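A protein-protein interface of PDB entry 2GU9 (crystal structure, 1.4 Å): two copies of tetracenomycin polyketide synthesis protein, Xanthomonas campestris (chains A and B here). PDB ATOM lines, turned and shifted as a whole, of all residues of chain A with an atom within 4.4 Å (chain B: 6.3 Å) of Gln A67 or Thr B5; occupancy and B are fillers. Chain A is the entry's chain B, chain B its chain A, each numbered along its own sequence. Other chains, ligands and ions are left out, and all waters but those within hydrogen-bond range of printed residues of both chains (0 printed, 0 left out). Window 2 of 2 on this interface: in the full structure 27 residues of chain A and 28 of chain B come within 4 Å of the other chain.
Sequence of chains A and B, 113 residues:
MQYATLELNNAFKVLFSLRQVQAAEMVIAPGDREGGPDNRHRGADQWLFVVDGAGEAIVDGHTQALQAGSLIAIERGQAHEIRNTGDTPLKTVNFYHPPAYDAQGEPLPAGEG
Among the printed residues, merely in contact across the chains: Ser A70 with Ala B4, Ala A65 with Tyr B3, Gly A69 with Thr B5, Gln A67 with Thr B5 and Gly A69 with Ala B4.
The side-chain hydroxyl (OH) of Tyr B3 sits at hydrogen-bond distance from the side-chain hydroxyl (OG1) of Thr B5 (2.6 Å). The backbone carbonyl oxygen of Val A50 lies within hydrogen-bond range of the backbone NH of Gly A69. The backbone NH (N) of Val A50 is in hydrogen-bond range of the backbone carbonyl oxygen (O) of Ser A70 (2.9 Å). The side-chain hydroxyl (OG) of Ser A70 lies within hydrogen-bond range of the backbone NH (N) of Gln A67 (2.8 Å).
Of the 8 printed residues of chain A, 4 touch a printed residue of chain B. Hydrophobic or aromatic side chains of chain B within 4 Å of the printed part of chain A: Tyr B3 and Leu B6. Among the printed residues, no Asp or Glu carboxylate lies within 4 Å of a Lys or Arg side-chain nitrogen of the other chain.
No position is printed for both chains.
Printed residues of chain B within 4 Å of Ala A65: Tyr B3. Of chain B, only Thr B5 comes within 4 Å of Gln A67. Of the printed residues of chain B, Gly A69 touches Ala B4 (3.99 Å), Thr B5 (3.8 Å) and Leu B6 (2.8 Å). Of the printed residues of chain A, Tyr B3 touches Ala A65 (3.5 Å) and Ser A70 (2.6 Å). Of chain A, only Gln A67 (3.8 Å) and Gly A69 (3.8 Å) come within 4 Å of Thr B5. Printed residues of chain A within 4 Å of Leu B6: Gly A69. Glu B7 touches none of the printed residues of chain A. Leu B8 touches none of the printed residues of chain A. The nearest residue of chain B that does not touch Gln A67 is Tyr B3 (4.1 Å). The nearest residue of chain A that does not touch Thr B5 is Ser A70 (4.3 Å).
OH of Tyr B3 sits at hydrogen-bond distance from OG of Ser A70, 2.6 Å away. The backbone carbonyl oxygen (O) of Gly A69 lies within hydrogen-bond range of the backbone NH (N) of Leu B6 (2.8 Å).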
ATOM      1  N   VAL A  50     -26.886  20.294  -2.863  1.00  0.00           N
ATOM      2  CA  VAL A  50     -25.814  20.378  -3.838  1.00  0.00           C
ATOM      3  C   VAL A  50     -24.443  20.153  -3.220  1.00  0.00           C
ATOM      4  O   VAL A  50     -23.991  20.922  -2.364  1.00  0.00           O
ATOM      5  CB  VAL A  50     -25.836  21.744  -4.545  1.00  0.00           C
ATOM      6  CG1 VAL A  50     -24.719  21.819  -5.594  1.00  0.00           C
ATOM      7  CG2 VAL A  50     -27.186  21.942  -5.198  1.00  0.00           C
ATOM      8  N   GLY A  53     -20.838  22.126  -7.896  1.00  0.00           N
ATOM      9  CA  GLY A  53     -21.382  22.660  -9.125  1.00  0.00           C
ATOM     10  C   GLY A  53     -22.331  23.805  -8.853  1.00  0.00           C
ATOM     11  O   GLY A  53     -22.560  24.176  -7.701  1.00  0.00           O
ATOM     12  N   ALA A  65     -31.414  30.063  -7.594  1.00  0.00           N
ATOM     13  CA  ALA A  65     -30.027  29.763  -7.909  1.00  0.00           C
ATOM     14  C   ALA A  65     -29.506  28.684  -6.968  1.00  0.00           C
ATOM     15  O   ALA A  65     -29.841  28.656  -5.783  1.00  0.00           O
ATOM     16  CB  ALA A  65     -29.170  31.018  -7.790  1.00  0.00           C
ATOM     17  N   LEU A  66     -28.667  27.809  -7.509  1.00  0.00           N
ATOM     18  CA  LEU A  66     -28.088  26.712  -6.756  1.00  0.00           C
ATOM     19  C   LEU A  66     -26.560  26.749  -6.803  1.00  0.00           C
ATOM     20  O   LEU A  66     -25.967  26.969  -7.857  1.00  0.00           O
ATOM     21  CB  LEU A  66     -28.580  25.380  -7.332  1.00  0.00           C
ATOM     22  CG  LEU A  66     -30.092  25.135  -7.313  1.00  0.00           C
ATOM     23  CD1 LEU A  66     -30.394  23.746  -7.865  1.00  0.00           C
ATOM     24  CD2 LEU A  66     -30.609  25.270  -5.884  1.00  0.00           C
ATOM     25  N   GLN A  67     -25.933  26.522  -5.654  1.00  0.00           N
ATOM     26  CA  GLN A  67     -24.477  26.522  -5.541  1.00  0.00           C
ATOM     27  C   GLN A  67     -24.081  25.443  -4.548  1.00  0.00           C
ATOM     28  O   GLN A  67     -24.940  24.851  -3.899  1.00  0.00           O
ATOM     29  CB  GLN A  67     -23.984  27.887  -5.040  1.00  0.00           C
ATOM     30  CG  GLN A  67     -24.625  28.319  -3.723  1.00  0.00           C
ATOM     31  CD  GLN A  67     -24.105  29.653  -3.210  1.00  0.00           C
ATOM     32  OE1 GLN A  67     -22.920  29.800  -2.910  1.00  0.00           O
ATOM     33  NE2 GLN A  67     -25.000  30.627  -3.093  1.00  0.00           N
ATOM     34  N   ALA A  68     -22.783  25.183  -4.426  1.00  0.00           N
ATOM     35  CA  ALA A  68     -22.322  24.176  -3.484  1.00  0.00           C
ATOM     36  C   ALA A  68     -22.835  24.531  -2.094  1.00  0.00           C
ATOM     37  O   ALA A  68     -22.618  25.646  -1.607  1.00  0.00           O
ATOM     38  CB  ALA A  68     -20.799  24.111  -3.484  1.00  0.00           C
ATOM     39  N   GLY A  69     -23.523  23.582  -1.464  1.00  0.00           N
ATOM     40  CA  GLY A  69     -24.058  23.812  -0.134  1.00  0.00           C
ATOM     41  C   GLY A  69     -25.532  24.164  -0.120  1.00  0.00           C
ATOM     42  O   GLY A  69     -26.152  24.203   0.945  1.00  0.00           O
ATOM     43  N   SER A  70     -26.101  24.428  -1.290  1.00  0.00           N
ATOM     44  CA  SER A  70     -27.515  24.768  -1.365  1.00  0.00           C
ATOM     45  C   SER A  70     -28.401  23.598  -0.991  1.00  0.00           C
ATOM     46  O   SER A  70     -28.126  22.449  -1.335  1.00  0.00           O
ATOM     47  CB  SER A  70     -27.924  25.208  -2.770  1.00  0.00           C
ATOM     48  OG  SER A  70     -27.299  26.412  -3.167  1.00  0.00           O
ATOM     49  N   TYR B   3     -35.550  27.412   0.777  1.00  0.00           N
ATOM     50  CA  TYR B   3     -34.154  27.357   0.379  1.00  0.00           C
ATOM     51  C   TYR B   3     -33.172  27.915   1.402  1.00  0.00           C
ATOM     52  O   TYR B   3     -33.485  28.839   2.148  1.00  0.00           O
ATOM     53  CB  TYR B   3     -33.981  28.113  -0.951  1.00  0.00           C
ATOM     54  CG  TYR B   3     -32.537  28.291  -1.367  1.00  0.00           C
ATOM     55  CD1 TYR B   3     -31.749  29.300  -0.811  1.00  0.00           C
ATOM     56  CD2 TYR B   3     -31.931  27.393  -2.242  1.00  0.00           C
ATOM     57  CE1 TYR B   3     -30.393  29.398  -1.108  1.00  0.00           C
ATOM     58  CE2 TYR B   3     -30.581  27.484  -2.542  1.00  0.00           C
ATOM     59  CZ  TYR B   3     -29.819  28.484  -1.967  1.00  0.00           C
ATOM     60  OH  TYR B   3     -28.470  28.542  -2.211  1.00  0.00           O
ATOM     61  N   ALA B   4     -31.974  27.344   1.425  1.00  0.00           N
ATOM     62  CA  ALA B   4     -30.918  27.808   2.310  1.00  0.00           C
ATOM     63  C   ALA B   4     -29.576  27.407   1.717  1.00  0.00           C
ATOM     64  O   ALA B   4     -29.477  26.400   1.019  1.00  0.00           O
ATOM     65  CB  ALA B   4     -31.075  27.195   3.693  1.00  0.00           C
ATOM     66  N   THR B   5     -28.558  28.220   1.965  1.00  0.00           N
ATOM     67  CA  THR B   5     -27.211  27.900   1.514  1.00  0.00           C
ATOM     68  C   THR B   5     -26.472  27.492   2.781  1.00  0.00           C
ATOM     69  O   THR B   5     -26.237  28.323   3.654  1.00  0.00           O
ATOM     70  CB  THR B   5     -26.482  29.121   0.915  1.00  0.00           C
ATOM     71  OG1 THR B   5     -27.238  29.643  -0.184  1.00  0.00           O
ATOM     72  CG2 THR B   5     -25.091  28.717   0.427  1.00  0.00           C
ATOM     73  N   LEU B   6     -26.121  26.216   2.900  1.00  0.00           N
ATOM     74  CA  LEU B   6     -25.406  25.760   4.083  1.00  0.00           C
ATOM     75  C   LEU B   6     -23.950  26.190   4.054  1.00  0.00           C
ATOM     76  O   LEU B   6     -23.251  25.983   3.064  1.00  0.00           O
ATOM     77  CB  LEU B   6     -25.475  24.238   4.217  1.00  0.00           C
ATOM     78  CG  LEU B   6     -26.772  23.645   4.772  1.00  0.00           C
ATOM     79  CD1 LEU B   6     -27.884  23.807   3.757  1.00  0.00           C
ATOM     80  CD2 LEU B   6     -26.551  22.174   5.108  1.00  0.00           C
ATOM     81  N   GLU B   7     -23.507  26.793   5.150  1.00  0.00           N
ATOM     82  CA  GLU B   7     -22.125  27.249   5.270  1.00  0.00           C
ATOM     83  C   GLU B   7     -21.287  26.178   5.960  1.00  0.00           C
ATOM     84  O   GLU B   7     -20.062  26.250   5.982  1.00  0.00           O
ATOM     85  CB  GLU B   7     -22.069  28.549   6.075  1.00  0.00           C
ATOM     86  CG  GLU B   7     -22.799  29.714   5.427  1.00  0.00           C
ATOM     87  CD  GLU B   7     -22.076  30.291   4.210  1.00  0.00           C
ATOM     88  OE1 GLU B   7     -22.658  31.171   3.529  1.00  0.00           O
ATOM     89  OE2 GLU B   7     -20.931  29.879   3.932  1.00  0.00           O
ATOM     90  N   LEU B   8     -21.961  25.186   6.530  1.00  0.00           N
ATOM     91  CA  LEU B   8     -21.288  24.092   7.215  1.00  0.00           C
ATOM     92  C   LEU B   8     -20.270  24.554   8.266  1.00  0.00           C
ATOM     93  O   LEU B   8     -19.117  24.125   8.271  1.00  0.00           O
ATOM     94  CB  LEU B   8     -20.631  23.160   6.179  1.00  0.00           C
ATOM     95  CG  LEU B   8     -21.614  22.468   5.217  1.00  0.00           C
ATOM     96  CD1 LEU B   8     -20.865  21.661   4.164  1.00  0.00           C
ATOM     97  CD2 LEU B   8     -22.553  21.573   6.014  1.00  0.00           C
ATOM     98  N   GLU B  25     -28.159  21.227   9.775  1.00  0.00           N
ATOM     99  CA  GLU B  25     -26.733  21.190   9.489  1.00  0.00           C
ATOM    100  C   GLU B  25     -26.058  20.754  10.781  1.00  0.00           C
ATOM    101  O   GLU B  25     -26.460  21.173  11.867  1.00  0.00           O
ATOM    102  CB  GLU B  25     -26.246  22.584   9.093  1.00  0.00           C
ATOM    103  CG  GLU B  25     -24.736  22.743   9.073  1.00  0.00           C
ATOM    104  CD  GLU B  25     -24.323  24.136   8.650  1.00  0.00           C
ATOM    105  OE1 GLU B  25     -24.665  24.536   7.520  1.00  0.00           O
ATOM    106  OE2 GLU B  25     -23.658  24.826   9.451  1.00  0.00           O
